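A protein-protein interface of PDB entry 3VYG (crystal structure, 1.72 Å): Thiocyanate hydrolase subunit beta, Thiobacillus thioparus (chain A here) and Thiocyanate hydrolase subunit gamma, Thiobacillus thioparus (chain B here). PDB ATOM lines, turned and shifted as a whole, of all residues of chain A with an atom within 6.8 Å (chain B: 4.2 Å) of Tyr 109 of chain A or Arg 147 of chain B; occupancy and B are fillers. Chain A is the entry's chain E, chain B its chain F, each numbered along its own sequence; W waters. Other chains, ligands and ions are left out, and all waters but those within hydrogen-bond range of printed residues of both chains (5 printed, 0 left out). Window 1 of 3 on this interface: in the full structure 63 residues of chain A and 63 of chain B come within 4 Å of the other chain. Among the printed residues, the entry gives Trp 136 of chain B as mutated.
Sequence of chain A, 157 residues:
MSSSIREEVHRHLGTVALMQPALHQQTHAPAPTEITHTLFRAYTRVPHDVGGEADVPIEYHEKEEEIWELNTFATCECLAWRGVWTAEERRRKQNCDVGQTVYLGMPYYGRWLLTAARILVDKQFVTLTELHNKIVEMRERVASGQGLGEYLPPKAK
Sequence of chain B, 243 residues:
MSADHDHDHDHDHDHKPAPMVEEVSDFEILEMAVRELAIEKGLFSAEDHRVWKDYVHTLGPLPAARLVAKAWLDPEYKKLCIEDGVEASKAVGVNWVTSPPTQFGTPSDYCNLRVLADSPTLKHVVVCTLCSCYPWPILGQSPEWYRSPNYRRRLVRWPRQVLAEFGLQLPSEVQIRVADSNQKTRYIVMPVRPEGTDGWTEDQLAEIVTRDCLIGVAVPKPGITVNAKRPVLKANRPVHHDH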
ATOM      1  N   LYS A  63     -23.219  30.238 -15.073  1.00  0.00           N
ATOM      2  CA  LYS A  63     -23.186  31.006 -16.324  1.00  0.00           C
ATOM      3  C   LYS A  63     -23.827  30.170 -17.442  1.00  0.00           C
ATOM      4  O   LYS A  63     -23.575  28.951 -17.535  1.00  0.00           O
ATOM      5  CB  LYS A  63     -21.776  31.456 -16.745  1.00  0.00           C
ATOM      6  CG  LYS A  63     -21.844  32.385 -18.009  1.00  0.00           C
ATOM      7  CD  LYS A  63     -20.405  32.767 -18.544  1.00  0.00           C
ATOM      8  CE  LYS A  63     -19.884  31.676 -19.544  1.00  0.00           C
ATOM      9  NZ  LYS A  63     -20.736  31.684 -20.834  1.00  0.00           N
ATOM     10  N   GLU A  65     -24.250  28.557 -21.021  1.00  0.00           N
ATOM     11  CA  GLU A  65     -23.288  28.195 -22.121  1.00  0.00           C
ATOM     12  C   GLU A  65     -23.613  29.023 -23.399  1.00  0.00           C
ATOM     13  O   GLU A  65     -24.794  29.064 -23.877  1.00  0.00           O
ATOM     14  CB  GLU A  65     -23.403  26.695 -22.279  1.00  0.00           C
ATOM     15  CG  GLU A  65     -22.423  26.023 -23.340  1.00  0.00           C
ATOM     16  CD  GLU A  65     -22.667  24.493 -23.505  1.00  0.00           C
ATOM     17  OE1 GLU A  65     -21.654  23.787 -23.598  1.00  0.00           O
ATOM     18  OE2 GLU A  65     -23.838  23.920 -23.577  1.00  0.00           O
ATOM     19  N   GLU A  66     -22.587  29.620 -23.980  1.00  0.00           N
ATOM     20  CA  GLU A  66     -22.716  30.292 -25.310  1.00  0.00           C
ATOM     21  C   GLU A  66     -22.708  29.213 -26.400  1.00  0.00           C
ATOM     22  O   GLU A  66     -22.093  28.142 -26.248  1.00  0.00           O
ATOM     23  CB  GLU A  66     -21.515  31.187 -25.610  1.00  0.00           C
ATOM     24  CG  GLU A  66     -21.275  32.400 -24.711  1.00  0.00           C
ATOM     25  CD  GLU A  66     -22.070  33.653 -25.141  1.00  0.00           C
ATOM     26  OE1 GLU A  66     -22.836  33.602 -26.164  1.00  0.00           O
ATOM     27  OE2 GLU A  66     -21.868  34.624 -24.396  1.00  0.00           O
ATOM     28  N   TRP A  68     -21.086  29.392 -29.081  1.00  0.00           N
ATOM     29  CA  TRP A  68     -19.708  29.255 -29.542  1.00  0.00           C
ATOM     30  C   TRP A  68     -18.878  28.425 -28.532  1.00  0.00           C
ATOM     31  O   TRP A  68     -17.895  27.762 -28.927  1.00  0.00           O
ATOM     32  CB  TRP A  68     -19.007  30.590 -29.837  1.00  0.00           C
ATOM     33  CG  TRP A  68     -18.634  31.438 -28.629  1.00  0.00           C
ATOM     34  CD1 TRP A  68     -19.288  32.499 -28.145  1.00  0.00           C
ATOM     35  CD2 TRP A  68     -17.416  31.338 -27.898  1.00  0.00           C
ATOM     36  NE1 TRP A  68     -18.607  33.083 -27.088  1.00  0.00           N
ATOM     37  CE2 TRP A  68     -17.467  32.335 -26.880  1.00  0.00           C
ATOM     38  CE3 TRP A  68     -16.332  30.477 -27.979  1.00  0.00           C
ATOM     39  CZ2 TRP A  68     -16.402  32.566 -25.986  1.00  0.00           C
ATOM     40  CZ3 TRP A  68     -15.286  30.649 -27.021  1.00  0.00           C
ATOM     41  CH2 TRP A  68     -15.323  31.698 -26.081  1.00  0.00           C
ATOM     42  N   GLU A  69     -19.260  28.455 -27.234  1.00  0.00           N
ATOM     43  CA  GLU A  69     -18.534  27.645 -26.223  1.00  0.00           C
ATOM     44  C   GLU A  69     -18.795  26.178 -26.429  1.00  0.00           C
ATOM     45  O   GLU A  69     -17.868  25.356 -26.425  1.00  0.00           O
ATOM     46  CB  GLU A  69     -18.988  28.103 -24.790  1.00  0.00           C
ATOM     47  CG  GLU A  69     -18.349  29.459 -24.460  1.00  0.00           C
ATOM     48  CD  GLU A  69     -18.879  29.959 -23.099  1.00  0.00           C
ATOM     49  OE1 GLU A  69     -19.989  29.521 -22.714  1.00  0.00           O
ATOM     50  OE2 GLU A  69     -18.143  30.677 -22.409  1.00  0.00           O
ATOM     51  N   LEU A  70     -20.056  25.804 -26.656  1.00  0.00           N
ATOM     52  CA  LEU A  70     -20.411  24.416 -26.906  1.00  0.00           C
ATOM     53  C   LEU A  70     -19.669  23.947 -28.201  1.00  0.00           C
ATOM     54  O   LEU A  70     -19.134  22.830 -28.237  1.00  0.00           O
ATOM     55  CB  LEU A  70     -21.927  24.306 -27.101  1.00  0.00           C
ATOM     56  CG  LEU A  70     -22.356  22.855 -27.450  1.00  0.00           C
ATOM     57  CD1 LEU A  70     -21.776  21.670 -26.560  1.00  0.00           C
ATOM     58  CD2 LEU A  70     -23.874  22.865 -27.786  1.00  0.00           C
ATOM     59  N   THR A  72     -16.922  25.116 -29.474  1.00  0.00           N
ATOM     60  CA  THR A  72     -15.430  25.032 -29.194  1.00  0.00           C
ATOM     61  C   THR A  72     -15.115  23.749 -28.422  1.00  0.00           C
ATOM     62  O   THR A  72     -14.185  22.981 -28.718  1.00  0.00           O
ATOM     63  CB  THR A  72     -15.016  26.252 -28.357  1.00  0.00           C
ATOM     64  OG1 THR A  72     -15.163  27.419 -29.160  1.00  0.00           O
ATOM     65  CG2 THR A  72     -13.542  26.049 -27.845  1.00  0.00           C
ATOM     66  N   PHE A  73     -15.926  23.443 -27.394  1.00  0.00           N
ATOM     67  CA  PHE A  73     -15.746  22.228 -26.641  1.00  0.00           C
ATOM     68  C   PHE A  73     -15.805  20.986 -27.547  1.00  0.00           C
ATOM     69  O   PHE A  73     -14.969  20.107 -27.449  1.00  0.00           O
ATOM     70  CB  PHE A  73     -16.895  22.189 -25.572  1.00  0.00           C
ATOM     71  CG  PHE A  73     -16.829  21.030 -24.588  1.00  0.00           C
ATOM     72  CD1 PHE A  73     -15.646  20.746 -23.903  1.00  0.00           C
ATOM     73  CD2 PHE A  73     -17.998  20.488 -24.127  1.00  0.00           C
ATOM     74  CE1 PHE A  73     -15.609  19.709 -22.887  1.00  0.00           C
ATOM     75  CE2 PHE A  73     -17.981  19.492 -23.077  1.00  0.00           C
ATOM     76  CZ  PHE A  73     -16.793  19.126 -22.474  1.00  0.00           C
ATOM     77  N   ALA A  74     -16.770  20.946 -28.451  1.00  0.00           N
ATOM     78  CA  ALA A  74     -16.937  19.807 -29.328  1.00  0.00           C
ATOM     79  C   ALA A  74     -15.771  19.762 -30.312  1.00  0.00           C
ATOM     80  O   ALA A  74     -15.229  18.662 -30.609  1.00  0.00           O
ATOM     81  CB  ALA A  74     -18.251  19.970 -30.036  1.00  0.00           C
ATOM     82  N   CYS A  76     -12.668  20.785 -29.761  1.00  0.00           N
ATOM     83  CA  CYS A  76     -11.489  20.318 -29.016  1.00  0.00           C
ATOM     84  C   CYS A  76     -11.519  18.794 -28.738  1.00  0.00           C
ATOM     85  O   CYS A  76     -10.525  18.060 -28.936  1.00  0.00           O
ATOM     86  CB  CYS A  76     -11.354  21.096 -27.670  1.00  0.00           C
ATOM     87  SG  CYS A  76     -10.845  22.802 -28.006  1.00  0.00           S
ATOM     88  N   TYR A 103      -3.783  33.825 -19.521  1.00  0.00           N
ATOM     89  CA  TYR A 103      -4.335  32.785 -18.682  1.00  0.00           C
ATOM     90  C   TYR A 103      -5.417  33.381 -17.755  1.00  0.00           C
ATOM     91  O   TYR A 103      -6.469  32.796 -17.588  1.00  0.00           O
ATOM     92  CB  TYR A 103      -3.242  32.198 -17.815  1.00  0.00           C
ATOM     93  CG  TYR A 103      -3.845  31.032 -17.007  1.00  0.00           C
ATOM     94  CD1 TYR A 103      -4.390  29.913 -17.657  1.00  0.00           C
ATOM     95  CD2 TYR A 103      -3.889  31.099 -15.574  1.00  0.00           C
ATOM     96  CE1 TYR A 103      -4.949  28.840 -16.928  1.00  0.00           C
ATOM     97  CE2 TYR A 103      -4.432  30.035 -14.862  1.00  0.00           C
ATOM     98  CZ  TYR A 103      -4.975  28.958 -15.518  1.00  0.00           C
ATOM     99  OH  TYR A 103      -5.589  27.936 -14.793  1.00  0.00           O
ATOM    100  N   MET A 106      -8.267  36.371 -20.232  1.00  0.00           N
ATOM    101  CA  MET A 106      -9.224  35.978 -21.239  1.00  0.00           C
ATOM    102  C   MET A 106     -10.158  34.988 -20.608  1.00  0.00           C
ATOM    103  O   MET A 106      -9.852  34.521 -19.472  1.00  0.00           O
ATOM    104  CB  MET A 106      -8.422  35.342 -22.411  1.00  0.00           C
ATOM    105  CG  MET A 106      -7.754  36.464 -23.211  1.00  0.00           C
ATOM    106  SD  MET A 106      -8.994  37.384 -24.250  1.00  0.00           S
ATOM    107  CE  MET A 106      -9.113  36.161 -25.602  1.00  0.00           C
ATOM    108  N   PRO A 107     -11.306  34.729 -21.232  1.00  0.00           N
ATOM    109  CA  PRO A 107     -12.251  33.777 -20.653  1.00  0.00           C
ATOM    110  C   PRO A 107     -11.788  32.337 -20.844  1.00  0.00           C
ATOM    111  O   PRO A 107     -11.017  32.014 -21.773  1.00  0.00           O
ATOM    112  CB  PRO A 107     -13.523  33.967 -21.460  1.00  0.00           C
ATOM    113  CG  PRO A 107     -13.294  35.292 -22.180  1.00  0.00           C
ATOM    114  CD  PRO A 107     -11.875  35.338 -22.446  1.00  0.00           C
ATOM    115  N   TYR A 108     -12.302  31.482 -19.962  1.00  0.00           N
ATOM    116  CA  TYR A 108     -11.983  30.021 -19.910  1.00  0.00           C
ATOM    117  C   TYR A 108     -12.175  29.442 -21.337  1.00  0.00           C
ATOM    118  O   TYR A 108     -11.213  28.928 -21.884  1.00  0.00           O
ATOM    119  CB  TYR A 108     -13.018  29.423 -18.926  1.00  0.00           C
ATOM    120  CG  TYR A 108     -13.101  27.920 -18.890  1.00  0.00           C
ATOM    121  CD1 TYR A 108     -12.285  27.194 -18.021  1.00  0.00           C
ATOM    122  CD2 TYR A 108     -14.081  27.248 -19.625  1.00  0.00           C
ATOM    123  CE1 TYR A 108     -12.418  25.787 -17.936  1.00  0.00           C
ATOM    124  CE2 TYR A 108     -14.223  25.853 -19.544  1.00  0.00           C
ATOM    125  CZ  TYR A 108     -13.335  25.167 -18.680  1.00  0.00           C
ATOM    126  OH  TYR A 108     -13.461  23.842 -18.575  1.00  0.00           O
ATOM    127  N   TYR A 109     -13.343  29.607 -21.982  1.00  0.00           N
ATOM    128  CA  TYR A 109     -13.410  28.967 -23.308  1.00  0.00           C
ATOM    129  C   TYR A 109     -12.754  29.756 -24.347  1.00  0.00           C
ATOM    130  O   TYR A 109     -12.498  29.175 -25.436  1.00  0.00           O
ATOM    131  CB  TYR A 109     -14.879  28.679 -23.684  1.00  0.00           C
ATOM    132  CG  TYR A 109     -15.426  27.361 -23.230  1.00  0.00           C
ATOM    133  CD1 TYR A 109     -16.550  27.312 -22.361  1.00  0.00           C
ATOM    134  CD2 TYR A 109     -14.788  26.107 -23.619  1.00  0.00           C
ATOM    135  CE1 TYR A 109     -17.070  26.056 -21.953  1.00  0.00           C
ATOM    136  CE2 TYR A 109     -15.307  24.892 -23.229  1.00  0.00           C
ATOM    137  CZ  TYR A 109     -16.427  24.866 -22.371  1.00  0.00           C
ATOM    138  OH  TYR A 109     -16.946  23.640 -22.023  1.00  0.00           O
ATOM    139  N   GLY A 110     -12.414  31.035 -24.070  1.00  0.00           N
ATOM    140  CA  GLY A 110     -11.580  31.802 -25.002  1.00  0.00           C
ATOM    141  C   GLY A 110     -10.259  31.060 -25.158  1.00  0.00           C
ATOM    142  O   GLY A 110      -9.722  31.019 -26.299  1.00  0.00           O
ATOM    143  N   ARG A 111      -9.686  30.576 -24.024  1.00  0.00           N
ATOM    144  CA  ARG A 111      -8.374  29.845 -24.082  1.00  0.00           C
ATOM    145  C   ARG A 111      -8.534  28.520 -24.827  1.00  0.00           C
ATOM    146  O   ARG A 111      -7.622  28.091 -25.579  1.00  0.00           O
ATOM    147  CB  ARG A 111      -7.762  29.641 -22.670  1.00  0.00           C
ATOM    148  CG  ARG A 111      -7.441  31.027 -22.089  1.00  0.00           C
ATOM    149  CD  ARG A 111      -6.807  30.959 -20.671  1.00  0.00           C
ATOM    150  NE  ARG A 111      -7.704  30.292 -19.710  1.00  0.00           N
ATOM    151  CZ  ARG A 111      -7.647  29.001 -19.365  1.00  0.00           C
ATOM    152  NH1 ARG A 111      -6.772  28.175 -19.943  1.00  0.00           N
ATOM    153  NH2 ARG A 111      -8.487  28.506 -18.436  1.00  0.00           N
ATOM    154  N   TRP A 112      -9.652  27.850 -24.610  1.00  0.00           N
ATOM    155  CA  TRP A 112      -9.835  26.564 -25.313  1.00  0.00           C
ATOM    156  C   TRP A 112      -9.875  26.862 -26.814  1.00  0.00           C
ATOM    157  O   TRP A 112      -9.248  26.086 -27.613  1.00  0.00           O
ATOM    158  CB  TRP A 112     -11.194  25.936 -24.985  1.00  0.00           C
ATOM    159  CG  TRP A 112     -11.342  25.256 -23.645  1.00  0.00           C
ATOM    160  CD1 TRP A 112     -11.170  25.791 -22.396  1.00  0.00           C
ATOM    161  CD2 TRP A 112     -11.629  23.851 -23.473  1.00  0.00           C
ATOM    162  NE1 TRP A 112     -11.390  24.774 -21.452  1.00  0.00           N
ATOM    163  CE2 TRP A 112     -11.628  23.588 -22.100  1.00  0.00           C
ATOM    164  CE3 TRP A 112     -11.825  22.795 -24.374  1.00  0.00           C
ATOM    165  CZ2 TRP A 112     -11.913  22.294 -21.569  1.00  0.00           C
ATOM    166  CZ3 TRP A 112     -12.091  21.508 -23.887  1.00  0.00           C
ATOM    167  CH2 TRP A 112     -12.179  21.275 -22.466  1.00  0.00           C
ATOM    168  N   LEU A 113     -10.524  27.953 -27.180  1.00  0.00           N
ATOM    169  CA  LEU A 113     -10.690  28.201 -28.666  1.00  0.00           C
ATOM    170  C   LEU A 113      -9.385  28.641 -29.258  1.00  0.00           C
ATOM    171  O   LEU A 113      -8.994  28.193 -30.369  1.00  0.00           O
ATOM    172  CB  LEU A 113     -11.777  29.306 -28.882  1.00  0.00           C
ATOM    173  CG  LEU A 113     -11.910  29.748 -30.370  1.00  0.00           C
ATOM    174  CD1 LEU A 113     -12.183  28.572 -31.355  1.00  0.00           C
ATOM    175  CD2 LEU A 113     -13.138  30.682 -30.419  1.00  0.00           C
ATOM    176  N   LEU A 114      -8.700  29.538 -28.571  1.00  0.00           N
ATOM    177  CA  LEU A 114      -7.374  29.953 -29.089  1.00  0.00           C
ATOM    178  C   LEU A 114      -6.421  28.779 -29.254  1.00  0.00           C
ATOM    179  O   LEU A 114      -5.635  28.715 -30.213  1.00  0.00           O
ATOM    180  CB  LEU A 114      -6.712  30.974 -28.127  1.00  0.00           C
ATOM    181  CG  LEU A 114      -7.335  32.359 -28.179  1.00  0.00           C
ATOM    182  CD1 LEU A 114      -6.951  33.201 -26.967  1.00  0.00           C
ATOM    183  CD2 LEU A 114      -7.038  33.138 -29.495  1.00  0.00           C
ATOM    184  N   THR A 115      -6.528  27.845 -28.337  1.00  0.00           N
ATOM    185  CA  THR A 115      -5.594  26.692 -28.305  1.00  0.00           C
ATOM    186  C   THR A 115      -5.971  25.696 -29.395  1.00  0.00           C
ATOM    187  O   THR A 115      -5.043  24.997 -29.939  1.00  0.00           O
ATOM    188  CB  THR A 115      -5.541  26.062 -26.886  1.00  0.00           C
ATOM    189  OG1 THR A 115      -5.147  27.135 -26.005  1.00  0.00           O
ATOM    190  CG2 THR A 115      -4.505  24.932 -26.770  1.00  0.00           C
ATOM    191  N   SER B 132     -10.336  22.224 -14.575  1.00  0.00           N
ATOM    192  CA  SER B 132     -11.820  22.134 -14.326  1.00  0.00           C
ATOM    193  C   SER B 132     -12.281  20.721 -14.459  1.00  0.00           C
ATOM    194  O   SER B 132     -13.475  20.484 -14.634  1.00  0.00           O
ATOM    195  CB  SER B 132     -12.624  22.988 -15.327  1.00  0.00           C
ATOM    196  OG  SER B 132     -12.185  22.561 -16.691  1.00  0.00           O
ATOM    197  N   TRP B 136     -17.780  14.584 -16.298  1.00  0.00           N
ATOM    198  CA  TRP B 136     -18.888  14.878 -17.223  1.00  0.00           C
ATOM    199  C   TRP B 136     -19.772  13.660 -17.619  1.00  0.00           C
ATOM    200  O   TRP B 136     -21.008  13.840 -17.741  1.00  0.00           O
ATOM    201  CB  TRP B 136     -18.300  15.493 -18.519  1.00  0.00           C
ATOM    202  CG  TRP B 136     -17.911  17.010 -18.380  1.00  0.00           C
ATOM    203  CD1 TRP B 136     -16.872  17.513 -17.688  1.00  0.00           C
ATOM    204  CD2 TRP B 136     -18.613  18.124 -18.956  1.00  0.00           C
ATOM    205  NE1 TRP B 136     -16.858  18.935 -17.797  1.00  0.00           N
ATOM    206  CE2 TRP B 136     -17.863  19.307 -18.635  1.00  0.00           C
ATOM    207  CE3 TRP B 136     -19.695  18.227 -19.854  1.00  0.00           C
ATOM    208  CZ2 TRP B 136     -18.211  20.576 -19.095  1.00  0.00           C
ATOM    209  CZ3 TRP B 136     -20.064  19.499 -20.286  1.00  0.00           C
ATOM    210  CH2 TRP B 136     -19.280  20.658 -19.928  1.00  0.00           C
ATOM    211  N   SER B 142     -19.758  21.076 -15.917  1.00  0.00           N
ATOM    212  CA  SER B 142     -19.100  21.620 -14.676  1.00  0.00           C
ATOM    213  C   SER B 142     -19.748  23.028 -14.477  1.00  0.00           C
ATOM    214  O   SER B 142     -20.045  23.732 -15.446  1.00  0.00           O
ATOM    215  CB  SER B 142     -17.619  21.704 -14.783  1.00  0.00           C
ATOM    216  OG  SER B 142     -17.202  22.412 -15.969  1.00  0.00           O
ATOM    217  N   PRO B 143     -19.967  23.415 -13.222  1.00  0.00           N
ATOM    218  CA  PRO B 143     -20.555  24.750 -13.027  1.00  0.00           C
ATOM    219  C   PRO B 143     -19.502  25.843 -13.332  1.00  0.00           C
ATOM    220  O   PRO B 143     -18.235  25.629 -13.212  1.00  0.00           O
ATOM    221  CB  PRO B 143     -20.840  24.817 -11.503  1.00  0.00           C
ATOM    222  CG  PRO B 143     -20.870  23.342 -11.058  1.00  0.00           C
ATOM    223  CD  PRO B 143     -19.862  22.616 -11.991  1.00  0.00           C
ATOM    224  N   GLU B 144     -20.016  27.032 -13.726  1.00  0.00           N
ATOM    225  CA  GLU B 144     -19.058  28.168 -13.891  1.00  0.00           C
ATOM    226  C   GLU B 144     -18.124  28.440 -12.730  1.00  0.00           C
ATOM    227  O   GLU B 144     -16.928  28.663 -12.904  1.00  0.00           O
ATOM    228  CB  GLU B 144     -19.870  29.427 -14.247  1.00  0.00           C
ATOM    229  CG  GLU B 144     -18.991  30.649 -14.677  1.00  0.00           C
ATOM    230  CD  GLU B 144     -18.387  30.590 -16.097  1.00  0.00           C
ATOM    231  OE1 GLU B 144     -18.675  29.585 -16.792  1.00  0.00           O
ATOM    232  OE2 GLU B 144     -17.706  31.593 -16.475  1.00  0.00           O
ATOM    233  N   TRP B 145     -18.633  28.408 -11.478  1.00  0.00           N
ATOM    234  CA  TRP B 145     -17.855  28.701 -10.336  1.00  0.00           C
ATOM    235  C   TRP B 145     -16.808  27.646 -10.039  1.00  0.00           C
ATOM    236  O   TRP B 145     -15.724  27.909  -9.449  1.00  0.00           O
ATOM    237  CB  TRP B 145     -18.805  28.874  -9.114  1.00  0.00           C
ATOM    238  CG  TRP B 145     -19.802  27.821  -8.868  1.00  0.00           C
ATOM    239  CD1 TRP B 145     -21.124  27.873  -9.232  1.00  0.00           C
ATOM    240  CD2 TRP B 145     -19.597  26.611  -8.191  1.00  0.00           C
ATOM    241  NE1 TRP B 145     -21.736  26.669  -8.788  1.00  0.00           N
ATOM    242  CE2 TRP B 145     -20.814  25.933  -8.134  1.00  0.00           C
ATOM    243  CE3 TRP B 145     -18.478  26.045  -7.533  1.00  0.00           C
ATOM    244  CZ2 TRP B 145     -20.943  24.640  -7.517  1.00  0.00           C
ATOM    245  CZ3 TRP B 145     -18.569  24.799  -6.969  1.00  0.00           C
ATOM    246  CH2 TRP B 145     -19.811  24.128  -6.885  1.00  0.00           C
ATOM    247  N   TYR B 146     -17.087  26.406 -10.527  1.00  0.00           N
ATOM    248  CA  TYR B 146     -16.117  25.302 -10.318  1.00  0.00           C
ATOM    249  C   TYR B 146     -14.866  25.493 -11.123  1.00  0.00           C
ATOM    250  O   TYR B 146     -13.775  25.148 -10.656  1.00  0.00           O
ATOM    251  CB  TYR B 146     -16.825  24.015 -10.680  1.00  0.00           C
ATOM    252  CG  TYR B 146     -16.019  22.794 -10.463  1.00  0.00           C
ATOM    253  CD1 TYR B 146     -16.041  22.035  -9.229  1.00  0.00           C
ATOM    254  CD2 TYR B 146     -15.256  22.329 -11.544  1.00  0.00           C
ATOM    255  CE1 TYR B 146     -15.242  20.836  -9.051  1.00  0.00           C
ATOM    256  CE2 TYR B 146     -14.550  21.153 -11.417  1.00  0.00           C
ATOM    257  CZ  TYR B 146     -14.478  20.439 -10.218  1.00  0.00           C
ATOM    258  OH  TYR B 146     -13.760  19.217 -10.012  1.00  0.00           O
ATOM    259  N   ARG B 147     -15.044  26.199 -12.266  1.00  0.00           N
ATOM    260  CA  ARG B 147     -13.941  26.584 -13.187  1.00  0.00           C
ATOM    261  C   ARG B 147     -13.185  27.853 -12.735  1.00  0.00           C
ATOM    262  O   ARG B 147     -12.121  28.151 -13.274  1.00  0.00           O
ATOM    263  CB  ARG B 147     -14.474  26.822 -14.569  1.00  0.00           C
ATOM    264  CG  ARG B 147     -15.337  25.728 -15.107  1.00  0.00           C
ATOM    265  CD  ARG B 147     -16.069  26.204 -16.387  1.00  0.00           C
ATOM    266  NE  ARG B 147     -17.021  25.184 -16.819  1.00  0.00           N
ATOM    267  CZ  ARG B 147     -17.851  25.329 -17.871  1.00  0.00           C
ATOM    268  NH1 ARG B 147     -17.797  26.429 -18.585  1.00  0.00           N
ATOM    269  NH2 ARG B 147     -18.761  24.390 -18.223  1.00  0.00           N
ATOM    270  N   SER B 148     -13.650  28.557 -11.688  1.00  0.00           N
ATOM    271  CA  SER B 148     -13.091  29.906 -11.394  1.00  0.00           C
ATOM    272  C   SER B 148     -11.739  29.770 -10.721  1.00  0.00           C
ATOM    273  O   SER B 148     -11.526  28.858  -9.878  1.00  0.00           O
ATOM    274  CB  SER B 148     -14.160  30.690 -10.468  1.00  0.00           C
ATOM    275  OG  SER B 148     -14.196  30.141  -9.138  1.00  0.00           O
ATOM    276  N   PRO B 149     -10.792  30.679 -11.032  1.00  0.00           N
ATOM    277  CA  PRO B 149      -9.582  30.678 -10.324  1.00  0.00           C
ATOM    278  C   PRO B 149      -9.795  30.828  -8.794  1.00  0.00           C
ATOM    279  O   PRO B 149      -9.046  30.222  -8.069  1.00  0.00           O
ATOM    280  CB  PRO B 149      -8.834  31.902 -10.888  1.00  0.00           C
ATOM    281  CG  PRO B 149      -9.395  32.095 -12.337  1.00  0.00           C
ATOM    282  CD  PRO B 149     -10.828  31.611 -12.220  1.00  0.00           C
ATOM    283  N   ARG B 152     -10.588  27.369  -7.337  1.00  0.00           N
ATOM    284  CA  ARG B 152      -9.396  26.580  -7.528  1.00  0.00           C
ATOM    285  C   ARG B 152      -8.256  26.964  -6.580  1.00  0.00           C
ATOM    286  O   ARG B 152      -7.454  26.111  -6.205  1.00  0.00           O
ATOM    287  CB  ARG B 152      -9.033  26.749  -9.002  1.00  0.00           C
ATOM    288  CG  ARG B 152      -9.945  26.024  -9.848  1.00  0.00           C
ATOM    289  CD  ARG B 152      -9.725  26.363 -11.389  1.00  0.00           C
ATOM    290  NE  ARG B 152      -8.323  26.144 -11.704  1.00  0.00           N
ATOM    291  CZ  ARG B 152      -7.529  26.974 -12.402  1.00  0.00           C
ATOM    292  NH1 ARG B 152      -8.088  27.946 -13.118  1.00  0.00           N
ATOM    293  NH2 ARG B 152      -6.260  26.734 -12.518  1.00  0.00           N
HETATM  294  O   HOH W   1     -19.979  27.586 -20.485  1.00  0.00           O
HETATM  295  O   HOH W   2     -20.696  28.041 -17.772  1.00  0.00           O
HETATM  296  O   HOH W   3     -10.021  23.847 -18.730  1.00  0.00           O
HETATM  297  O   HOH W   4      -7.763  30.454 -15.080  1.00  0.00           O
HETATM  298  O   HOH W   5     -22.703  27.353 -14.375  1.00  0.00           O
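The side-chain hydroxyl (OH) of Tyr 103 of chain A sits at hydrogen-bond distance from the guanidinium group (NH2) of Arg 152 of chain B (2.7 Å). OH of Tyr 108 of chain A lies within hydrogen-bond range of OG of Ser 132 of chain B, at 2.6 Å.
NZ of Lys 63 of chain A is in salt-bridge range of OE1 of Glu 69 of chain A, 3.0 Å away. OG of Ser 142 of chain B is in hydrogen-bond range of NE of Arg 147 of chain B (2.9 Å). OE1 of Glu 144 of chain B is in salt-bridge range of NH1 of Arg 147 of chain B (3.7 Å).
Among the printed residues, merely in contact across the chains: Lys 63 of chain A with Glu 144 of chain B (3.5 Å), Phe 73 of chain A with Trp 136 of chain B (3.5 Å), Tyr 108 of chain A with Arg 147 of chain B (3.7 Å) and Tyr 109 of chain A with Arg 147 of chain B (3.5 Å).
Of the printed residues of chain B, Lys 63 of chain A touches Glu 144. Of the printed residues of chain B, Tyr 103 of chain A touches Arg 152 (2.7 Å). Of the printed residues of chain B, Tyr 108 of chain A touches Ser 132 and Arg 147. Tyr 109 of chain A touches just one residue of chain B: Arg 147 (3.5 Å). Printed residues of chain A within 4 Å of Trp 136 of chain B: Phe 73. Of the printed residues of chain A, Glu 144 of chain B touches Lys 63 (3.5 Å). The nearest residue of chain A that does not touch Arg 147 of chain B is Glu 69 of chain A (5.6 Å).
Hydrophobic or aromatic side chains of chain B that line the printed part of chain A: Trp 136. Hydrophobic or aromatic side chains of chain A within 4 Å of the printed part of chain B: Phe 73, Tyr 103, Tyr 108 and Tyr 109.
Water W2 lies within hydrogen-bond range of OE1 of Glu 144 of chain B (2.7 Å), O of Lys 63 of chain A (3.0 Å) and NH1 of Arg 147 of chain B (3.4 Å). Water W5 lies within hydrogen-bond range of N of Glu 144 of chain B (2.8 Å) and N of Lys 63 of chain A (3.0 Å). Water W1 bridges OE1 of Glu 69 of chain A (3.0 Å) and NH1 of Arg 147 of chain B (3.1 Å). Water W3 lies within hydrogen-bond range of the indole nitrogen of Trp 112 of chain A (3.2 Å), the side-chain hydroxyl of Ser 132 of chain B (3.2 Å) and the side-chain hydroxyl of Tyr 108 of chain A (3.4 Å). Water W4 lies within hydrogen-bond range of the guanidinium group of Arg 152 of chain B (3.2 Å) and the side-chain hydroxyl of Tyr 103 of chain A (3.3 Å).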
